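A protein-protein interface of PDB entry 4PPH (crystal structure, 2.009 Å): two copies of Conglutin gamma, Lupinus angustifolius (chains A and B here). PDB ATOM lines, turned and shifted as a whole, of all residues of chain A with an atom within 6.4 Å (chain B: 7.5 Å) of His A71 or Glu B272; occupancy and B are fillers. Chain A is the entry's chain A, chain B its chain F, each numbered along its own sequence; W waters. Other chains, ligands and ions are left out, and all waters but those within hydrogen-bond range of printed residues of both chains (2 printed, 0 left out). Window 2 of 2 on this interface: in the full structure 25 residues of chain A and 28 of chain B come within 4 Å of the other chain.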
ATOM      1  N   PHE A  69       5.378  12.155  11.302  1.00  0.00           N
ATOM      2  CA  PHE A  69       4.718  12.019  12.601  1.00  0.00           C
ATOM      3  C   PHE A  69       3.833  10.785  12.642  1.00  0.00           C
ATOM      4  O   PHE A  69       3.388  10.289  11.619  1.00  0.00           O
ATOM      5  CB  PHE A  69       3.924  13.298  12.971  1.00  0.00           C
ATOM      6  CG  PHE A  69       2.860  13.711  11.967  1.00  0.00           C
ATOM      7  CD1 PHE A  69       1.605  13.121  11.968  1.00  0.00           C
ATOM      8  CD2 PHE A  69       3.093  14.749  11.074  1.00  0.00           C
ATOM      9  CE1 PHE A  69       0.617  13.519  11.073  1.00  0.00           C
ATOM     10  CE2 PHE A  69       2.100  15.157  10.172  1.00  0.00           C
ATOM     11  CZ  PHE A  69       0.866  14.533  10.177  1.00  0.00           C
ATOM     12  N   CYS A  70       3.596  10.279  13.839  1.00  0.00           N
ATOM     13  CA  CYS A  70       2.799   9.082  13.990  1.00  0.00           C
ATOM     14  C   CYS A  70       1.399   9.323  13.448  1.00  0.00           C
ATOM     15  O   CYS A  70       0.841  10.400  13.626  1.00  0.00           O
ATOM     16  CB  CYS A  70       2.752   8.658  15.452  1.00  0.00           C
ATOM     17  SG  CYS A  70       2.338   6.938  15.685  1.00  0.00           S
ATOM     18  N   HIS A  71       0.861   8.326  12.758  1.00  0.00           N
ATOM     19  CA  HIS A  71      -0.459   8.400  12.128  1.00  0.00           C
ATOM     20  C   HIS A  71      -0.467   9.293  10.897  1.00  0.00           C
ATOM     21  O   HIS A  71      -1.531   9.681  10.425  1.00  0.00           O
ATOM     22  CB  HIS A  71      -1.527   8.892  13.112  1.00  0.00           C
ATOM     23  CG  HIS A  71      -1.503   8.196  14.435  1.00  0.00           C
ATOM     24  ND1 HIS A  71      -1.742   6.847  14.571  1.00  0.00           N
ATOM     25  CD2 HIS A  71      -1.294   8.667  15.685  1.00  0.00           C
ATOM     26  CE1 HIS A  71      -1.668   6.513  15.844  1.00  0.00           C
ATOM     27  NE2 HIS A  71      -1.401   7.600  16.543  1.00  0.00           N
ATOM     28  N   SER A  72       0.706   9.655  10.395  1.00  0.00           N
ATOM     29  CA  SER A  72       0.760  10.399   9.157  1.00  0.00           C
ATOM     30  C   SER A  72       0.469   9.494   7.953  1.00  0.00           C
ATOM     31  O   SER A  72       0.458   8.267   8.052  1.00  0.00           O
ATOM     32  CB  SER A  72       2.121  11.064   9.003  1.00  0.00           C
ATOM     33  OG  SER A  72       3.125  10.059   8.987  1.00  0.00           O
ATOM     34  N   THR A  73       0.240  10.117   6.809  1.00  0.00           N
ATOM     35  CA  THR A  73       0.071   9.387   5.568  1.00  0.00           C
ATOM     36  C   THR A  73       1.347   8.650   5.219  1.00  0.00           C
ATOM     37  O   THR A  73       1.302   7.598   4.595  1.00  0.00           O
ATOM     38  CB  THR A  73      -0.311  10.315   4.414  1.00  0.00           C
ATOM     39  OG1 THR A  73       0.647  11.381   4.312  1.00  0.00           O
ATOM     40  CG2 THR A  73      -1.693  10.899   4.636  1.00  0.00           C
ATOM     41  N   GLN A  74       2.494   9.206   5.597  1.00  0.00           N
ATOM     42  CA  GLN A  74       3.751   8.514   5.386  1.00  0.00           C
ATOM     43  C   GLN A  74       3.875   7.234   6.203  1.00  0.00           C
ATOM     44  O   GLN A  74       4.321   6.225   5.695  1.00  0.00           O
ATOM     45  CB  GLN A  74       4.925   9.440   5.689  1.00  0.00           C
ATOM     46  CG  GLN A  74       5.032  10.639   4.735  1.00  0.00           C
ATOM     47  CD  GLN A  74       4.478  11.899   5.348  1.00  0.00           C
ATOM     48  OE1 GLN A  74       3.593  11.853   6.180  1.00  0.00           O
ATOM     49  NE2 GLN A  74       5.025  13.030   4.962  1.00  0.00           N
ATOM     50  N   CYS A  75       3.465   7.267   7.457  1.00  0.00           N
ATOM     51  CA  CYS A  75       3.488   6.079   8.292  1.00  0.00           C
ATOM     52  C   CYS A  75       2.476   5.057   7.807  1.00  0.00           C
ATOM     53  O   CYS A  75       2.672   3.863   7.928  1.00  0.00           O
ATOM     54  CB  CYS A  75       3.212   6.455   9.727  1.00  0.00           C
ATOM     55  SG  CYS A  75       4.472   7.532  10.344  1.00  0.00           S
ATOM     56  N   SER A  76       1.365   5.547   7.298  1.00  0.00           N
ATOM     57  CA  SER A  76       0.376   4.691   6.670  1.00  0.00           C
ATOM     58  C   SER A  76       0.916   3.935   5.441  1.00  0.00           C
ATOM     59  O   SER A  76       0.745   2.731   5.333  1.00  0.00           O
ATOM     60  CB  SER A  76      -0.839   5.537   6.290  1.00  0.00           C
ATOM     61  OG  SER A  76      -1.816   4.731   5.669  1.00  0.00           O
ATOM     62  N   THR A  80       3.145   1.135   9.095  1.00  0.00           N
ATOM     63  CA  THR A  80       3.431   1.100  10.517  1.00  0.00           C
ATOM     64  C   THR A  80       2.512   2.046  11.264  1.00  0.00           C
ATOM     65  O   THR A  80       2.418   3.244  10.942  1.00  0.00           O
ATOM     66  CB  THR A  80       4.860   1.481  10.834  1.00  0.00           C
ATOM     67  OG1 THR A  80       4.972   1.658  12.250  1.00  0.00           O
ATOM     68  CG2 THR A  80       5.263   2.775  10.119  1.00  0.00           C
ATOM     69  N   HIS A  81       1.814   1.501  12.253  1.00  0.00           N
ATOM     70  CA  HIS A  81       0.936   2.315  13.093  1.00  0.00           C
ATOM     71  C   HIS A  81       1.317   2.207  14.589  1.00  0.00           C
ATOM     72  O   HIS A  81       0.522   2.541  15.472  1.00  0.00           O
ATOM     73  CB  HIS A  81      -0.537   1.959  12.818  1.00  0.00           C
ATOM     74  CG  HIS A  81      -1.002   2.366  11.443  1.00  0.00           C
ATOM     75  ND1 HIS A  81      -1.600   3.585  11.186  1.00  0.00           N
ATOM     76  CD2 HIS A  81      -0.912   1.736  10.245  1.00  0.00           C
ATOM     77  CE1 HIS A  81      -1.882   3.674   9.897  1.00  0.00           C
ATOM     78  NE2 HIS A  81      -1.475   2.566   9.303  1.00  0.00           N
ATOM     79  N   CYS A  83       3.680   3.820  17.392  1.00  0.00           N
ATOM     80  CA  CYS A  83       4.401   5.080  17.578  1.00  0.00           C
ATOM     81  C   CYS A  83       5.784   4.893  18.143  1.00  0.00           C
ATOM     82  O   CYS A  83       6.055   3.937  18.860  1.00  0.00           O
ATOM     83  CB  CYS A  83       3.626   6.020  18.482  1.00  0.00           C
ATOM     84  SG  CYS A  83       2.163   6.614  17.680  1.00  0.00           S
ATOM     85  N   ASN A  99       6.830  10.724  19.299  1.00  0.00           N
ATOM     86  CA  ASN A  99       5.656  10.843  18.454  1.00  0.00           C
ATOM     87  C   ASN A  99       5.964  10.662  16.992  1.00  0.00           C
ATOM     88  O   ASN A  99       5.330  11.284  16.147  1.00  0.00           O
ATOM     89  CB  ASN A  99       4.992  12.204  18.657  1.00  0.00           C
ATOM     90  CG  ASN A  99       4.722  12.506  20.120  1.00  0.00           C
ATOM     91  OD1 ASN A  99       4.093  11.711  20.812  1.00  0.00           O
ATOM     92  ND2 ASN A  99       5.234  13.647  20.609  1.00  0.00           N
ATOM     93  N   THR A 100       6.938   9.808  16.691  1.00  0.00           N
ATOM     94  CA  THR A 100       7.201   9.405  15.315  1.00  0.00           C
ATOM     95  C   THR A 100       6.675   7.985  15.144  1.00  0.00           C
ATOM     96  O   THR A 100       5.932   7.525  16.004  1.00  0.00           O
ATOM     97  CB  THR A 100       8.705   9.494  14.976  1.00  0.00           C
ATOM     98  OG1 THR A 100       9.477   9.027  16.081  1.00  0.00           O
ATOM     99  CG2 THR A 100       9.093  10.913  14.759  1.00  0.00           C
ATOM    100  N   CYS A 101       7.026   7.289  14.052  1.00  0.00           N
ATOM    101  CA  CYS A 101       6.606   5.885  13.931  1.00  0.00           C
ATOM    102  C   CYS A 101       7.767   4.924  13.804  1.00  0.00           C
ATOM    103  O   CYS A 101       8.830   5.234  13.253  1.00  0.00           O
ATOM    104  CB  CYS A 101       5.611   5.675  12.776  1.00  0.00           C
ATOM    105  SG  CYS A 101       5.948   6.455  11.220  1.00  0.00           S
ATOM    106  N   LEU B 230      -3.426  16.027   8.336  1.00  0.00           N
ATOM    107  CA  LEU B 230      -4.187  14.839   8.036  1.00  0.00           C
ATOM    108  C   LEU B 230      -3.621  13.642   8.808  1.00  0.00           C
ATOM    109  O   LEU B 230      -2.432  13.396   8.767  1.00  0.00           O
ATOM    110  CB  LEU B 230      -4.146  14.574   6.533  1.00  0.00           C
ATOM    111  CG  LEU B 230      -4.843  13.337   5.974  1.00  0.00           C
ATOM    112  CD1 LEU B 230      -6.351  13.394   6.213  1.00  0.00           C
ATOM    113  CD2 LEU B 230      -4.504  13.188   4.493  1.00  0.00           C
ATOM    114  N   THR B 231      -4.474  12.904   9.522  1.00  0.00           N
ATOM    115  CA  THR B 231      -4.044  11.663  10.151  1.00  0.00           C
ATOM    116  C   THR B 231      -4.878  10.528   9.597  1.00  0.00           C
ATOM    117  O   THR B 231      -6.025  10.722   9.183  1.00  0.00           O
ATOM    118  CB  THR B 231      -4.173  11.669  11.684  1.00  0.00           C
ATOM    119  OG1 THR B 231      -5.436  12.220  12.043  1.00  0.00           O
ATOM    120  CG2 THR B 231      -3.051  12.479  12.334  1.00  0.00           C
ATOM    121  N   ILE B 232      -4.277   9.342   9.615  1.00  0.00           N
ATOM    122  CA  ILE B 232      -4.819   8.164   8.966  1.00  0.00           C
ATOM    123  C   ILE B 232      -4.986   7.054   9.998  1.00  0.00           C
ATOM    124  O   ILE B 232      -4.051   6.750  10.711  1.00  0.00           O
ATOM    125  CB  ILE B 232      -3.872   7.683   7.830  1.00  0.00           C
ATOM    126  CG1 ILE B 232      -3.605   8.800   6.829  1.00  0.00           C
ATOM    127  CG2 ILE B 232      -4.457   6.507   7.107  1.00  0.00           C
ATOM    128  CD1 ILE B 232      -4.859   9.259   6.122  1.00  0.00           C
ATOM    129  N   SER B 233      -6.160   6.445  10.095  1.00  0.00           N
ATOM    130  CA  SER B 233      -6.348   5.360  11.057  1.00  0.00           C
ATOM    131  C   SER B 233      -5.739   4.044  10.578  1.00  0.00           C
ATOM    132  O   SER B 233      -5.309   3.921   9.420  1.00  0.00           O
ATOM    133  CB  SER B 233      -7.822   5.164  11.371  1.00  0.00           C
ATOM    134  OG  SER B 233      -8.468   4.565  10.284  1.00  0.00           O
ATOM    135  N   LYS B 234      -5.722   3.044  11.459  1.00  0.00           N
ATOM    136  CA  LYS B 234      -5.153   1.743  11.092  1.00  0.00           C
ATOM    137  C   LYS B 234      -5.959   1.100   9.963  1.00  0.00           C
ATOM    138  O   LYS B 234      -5.460   0.198   9.302  1.00  0.00           O
ATOM    139  CB  LYS B 234      -5.081   0.791  12.300  1.00  0.00           C
ATOM    140  CG  LYS B 234      -4.250   1.343  13.459  1.00  0.00           C
ATOM    141  CD  LYS B 234      -4.224   0.442  14.702  1.00  0.00           C
ATOM    142  CE  LYS B 234      -3.731   1.259  15.902  1.00  0.00           C
ATOM    143  NZ  LYS B 234      -2.331   1.754  15.826  1.00  0.00           N
ATOM    144  N   GLU B 237      -8.551   5.198   7.032  1.00  0.00           N
ATOM    145  CA  GLU B 237      -9.527   6.286   6.971  1.00  0.00           C
ATOM    146  C   GLU B 237      -8.886   7.654   7.206  1.00  0.00           C
ATOM    147  O   GLU B 237      -7.883   7.749   7.903  1.00  0.00           O
ATOM    148  CB  GLU B 237     -10.611   6.083   8.023  1.00  0.00           C
ATOM    149  CG  GLU B 237     -11.329   4.758   7.996  1.00  0.00           C
ATOM    150  CD  GLU B 237     -11.879   4.397   9.369  1.00  0.00           C
ATOM    151  OE1 GLU B 237     -11.079   4.244  10.308  1.00  0.00           O
ATOM    152  OE2 GLU B 237     -13.105   4.264   9.510  1.00  0.00           O
ATOM    153  N   PHE B 239      -8.681  11.381   8.738  1.00  0.00           N
ATOM    154  CA  PHE B 239      -9.091  12.128   9.915  1.00  0.00           C
ATOM    155  C   PHE B 239      -8.453  13.494   9.967  1.00  0.00           C
ATOM    156  O   PHE B 239      -7.306  13.664   9.577  1.00  0.00           O
ATOM    157  CB  PHE B 239      -8.716  11.363  11.197  1.00  0.00           C
ATOM    158  CG  PHE B 239      -9.681  10.250  11.557  1.00  0.00           C
ATOM    159  CD1 PHE B 239      -9.561   8.995  11.001  1.00  0.00           C
ATOM    160  CD2 PHE B 239     -10.700  10.474  12.453  1.00  0.00           C
ATOM    161  CE1 PHE B 239     -10.454   7.994  11.317  1.00  0.00           C
ATOM    162  CE2 PHE B 239     -11.579   9.487  12.778  1.00  0.00           C
ATOM    163  CZ  PHE B 239     -11.449   8.233  12.205  1.00  0.00           C
ATOM    164  N   GLN B 241      -8.381  17.017  12.966  1.00  0.00           N
ATOM    165  CA  GLN B 241      -8.602  17.393  14.348  1.00  0.00           C
ATOM    166  C   GLN B 241      -9.459  18.665  14.463  1.00  0.00           C
ATOM    167  O   GLN B 241      -9.057  19.750  14.068  1.00  0.00           O
ATOM    168  CB  GLN B 241      -7.247  17.582  15.037  1.00  0.00           C
ATOM    169  CG  GLN B 241      -7.294  18.139  16.438  1.00  0.00           C
ATOM    170  CD  GLN B 241      -8.063  17.263  17.428  1.00  0.00           C
ATOM    171  OE1 GLN B 241      -8.177  16.035  17.254  1.00  0.00           O
ATOM    172  NE2 GLN B 241      -8.612  17.904  18.477  1.00  0.00           N
ATOM    173  N   GLY B 271      -0.619  14.666  19.818  1.00  0.00           N
ATOM    174  CA  GLY B 271      -0.124  14.026  18.611  1.00  0.00           C
ATOM    175  C   GLY B 271      -0.664  12.622  18.391  1.00  0.00           C
ATOM    176  O   GLY B 271       0.080  11.630  18.445  1.00  0.00           O
ATOM    177  N   GLU B 272      -1.960  12.543  18.102  1.00  0.00           N
ATOM    178  CA  GLU B 272      -2.635  11.272  17.884  1.00  0.00           C
ATOM    179  C   GLU B 272      -3.544  11.487  16.672  1.00  0.00           C
ATOM    180  O   GLU B 272      -3.461  12.531  16.044  1.00  0.00           O
ATOM    181  CB  GLU B 272      -3.371  10.870  19.176  1.00  0.00           C
ATOM    182  CG  GLU B 272      -3.570   9.370  19.391  1.00  0.00           C
ATOM    183  CD  GLU B 272      -4.777   8.734  18.698  1.00  0.00           C
ATOM    184  OE1 GLU B 272      -5.612   9.451  18.104  1.00  0.00           O
ATOM    185  OE2 GLU B 272      -4.885   7.477  18.758  1.00  0.00           O
ATOM    186  N   ILE B 273      -4.404  10.533  16.334  1.00  0.00           N
ATOM    187  CA  ILE B 273      -5.304  10.655  15.173  1.00  0.00           C
ATOM    188  C   ILE B 273      -6.374  11.742  15.429  1.00  0.00           C
ATOM    189  O   ILE B 273      -6.869  11.886  16.552  1.00  0.00           O
ATOM    190  CB  ILE B 273      -6.016   9.291  14.854  1.00  0.00           C
ATOM    191  CG1 ILE B 273      -5.022   8.158  14.704  1.00  0.00           C
ATOM    192  CG2 ILE B 273      -6.804   9.374  13.558  1.00  0.00           C
ATOM    193  CD1 ILE B 273      -5.698   6.891  14.252  1.00  0.00           C
ATOM    194  N   GLY B 274      -6.755  12.488  14.393  1.00  0.00           N
ATOM    195  CA  GLY B 274      -7.777  13.506  14.548  1.00  0.00           C
ATOM    196  C   GLY B 274      -9.055  12.877  15.054  1.00  0.00           C
ATOM    197  O   GLY B 274      -9.192  11.658  15.023  1.00  0.00           O
ATOM    198  N   GLY B 275      -9.972  13.691  15.564  1.00  0.00           N
ATOM    199  CA  GLY B 275     -11.191  13.155  16.124  1.00  0.00           C
ATOM    200  C   GLY B 275     -12.323  13.189  15.139  1.00  0.00           C
ATOM    201  O   GLY B 275     -13.365  12.599  15.387  1.00  0.00           O
ATOM    202  N   ASP B 336      -7.195  21.890  14.204  1.00  0.00           N
ATOM    203  CA  ASP B 336      -6.004  21.513  14.942  1.00  0.00           C
ATOM    204  C   ASP B 336      -5.176  22.711  15.405  1.00  0.00           C
ATOM    205  O   ASP B 336      -4.895  23.624  14.631  1.00  0.00           O
ATOM    206  CB  ASP B 336      -5.146  20.586  14.068  1.00  0.00           C
ATOM    207  CG  ASP B 336      -3.975  19.962  14.828  1.00  0.00           C
ATOM    208  OD1 ASP B 336      -4.169  18.893  15.447  1.00  0.00           O
ATOM    209  OD2 ASP B 336      -2.861  20.528  14.790  1.00  0.00           O
ATOM    210  N   SER B 392       0.971  15.126   4.140  1.00  0.00           N
ATOM    211  CA  SER B 392       0.037  14.676   5.164  1.00  0.00           C
ATOM    212  C   SER B 392      -0.817  15.795   5.710  1.00  0.00           C
ATOM    213  O   SER B 392      -0.825  16.040   6.917  1.00  0.00           O
ATOM    214  CB  SER B 392       0.770  14.022   6.327  1.00  0.00           C
ATOM    215  OG  SER B 392      -0.137  13.257   7.100  1.00  0.00           O
HETATM  216  O   HOH W   1      -3.228   2.917   7.181  1.00  0.00           O
HETATM  217  O   HOH W   2      -3.181   5.033  12.971  1.00  0.00           O
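No position is printed for both chains.
Hydrophobic or aromatic side chains of chain A within 4 Å of the printed part of chain B: Phe A69, His A71 and His A81.
His A71 touches just these residues of chain B: Thr B231, Ile B232, Glu B272 and Ile B273.
Glu B272 touches one residue of chain A.
Printed residues of chain A within 4 Å of Lys B234: His A81 (3.0 Å).
Of the printed residues of chain B, Phe A69 touches Leu B230 and Ser B392.
Printed residues of chain B within 4 Å of Ser A72: Ser B392 (3.6 Å).
Printed residues of chain A within 4 Å of Ile B273: His A71.
Cys A101 touches none of the printed residues of chain B.
The nearest residue of chain B that does not touch His A71 is Leu B230 (4.2 Å).
The nearest residue of chain A that does not touch Glu B272 is Cys A70 (5.4 Å).
Water W1 lies within hydrogen-bond range of OG of Ser A76 (2.8 Å), NE2 of His A81 (2.8 Å) and O of Ser B233 (3.2 Å).
Water W2 lies within hydrogen-bond range of a ring nitrogen (ND1) of His A81 (2.8 Å), a ring nitrogen (ND1) of His A71 (2.8 Å) and the backbone carbonyl oxygen of Ile B232 (3.0 Å).
OG of Ser A72 sits close to OE1 of Gln A74, at 3.4 Å.
The side-chain hydroxyl (OG) of Ser A72 is in hydrogen-bond range of the side-chain sulfur (SG) of Cys A75, 3.2 Å away.
The side-chain hydroxyl of Thr B231 is in hydrogen-bond range of the backbone NH of Gly B274, 2.7 Å away.
The side-chain carboxylate (OE1) of Glu B237 sits at hydrogen-bond distance from the side-chain hydroxyl (OG) of Ser B233 (2.6 Å).
The side-chain sulfur (SG) of Cys A70 is disulfide-bonded to the side-chain sulfur (SG) of Cys A83 (2.0 Å).
The side-chain sulfur (SG) of Cys A75 is disulfide-bonded to the side-chain sulfur (SG) of Cys A101.
Among the printed residues, merely in contact across the chains: Phe A69 with Leu B230 (3.8 Å), Phe A69 with Ser B392 (3.5 Å), His A71 with Thr B231 (3.2 Å), His A71 with Glu B272 (3.7 Å), His A71 with Ile B273 (3.5 Å), Ser A72 with Ser B392 (3.6 Å), Thr A73 with Leu B230 (3.6 Å), Thr A73 with Ile B232 (3.6 Å), Gln A74 with Ser B392 (3.6 Å), Ser A76 with Ile B232 (3.5 Å), His A81 with Ile B232 (3.9 Å) and His A81 with Ser B233 (3.5 Å).
The backbone carbonyl oxygen of His A71 is in hydrogen-bond range of the backbone NH of Ile B232 (2.9 Å).
N of Thr A73 sits at hydrogen-bond distance from OG of Ser B392 (3.2 Å).
The backbone carbonyl oxygen (O) of His A81 sits at hydrogen-bond distance from the side-chain amino group (NZ) of Lys B234 (3.0 Å).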
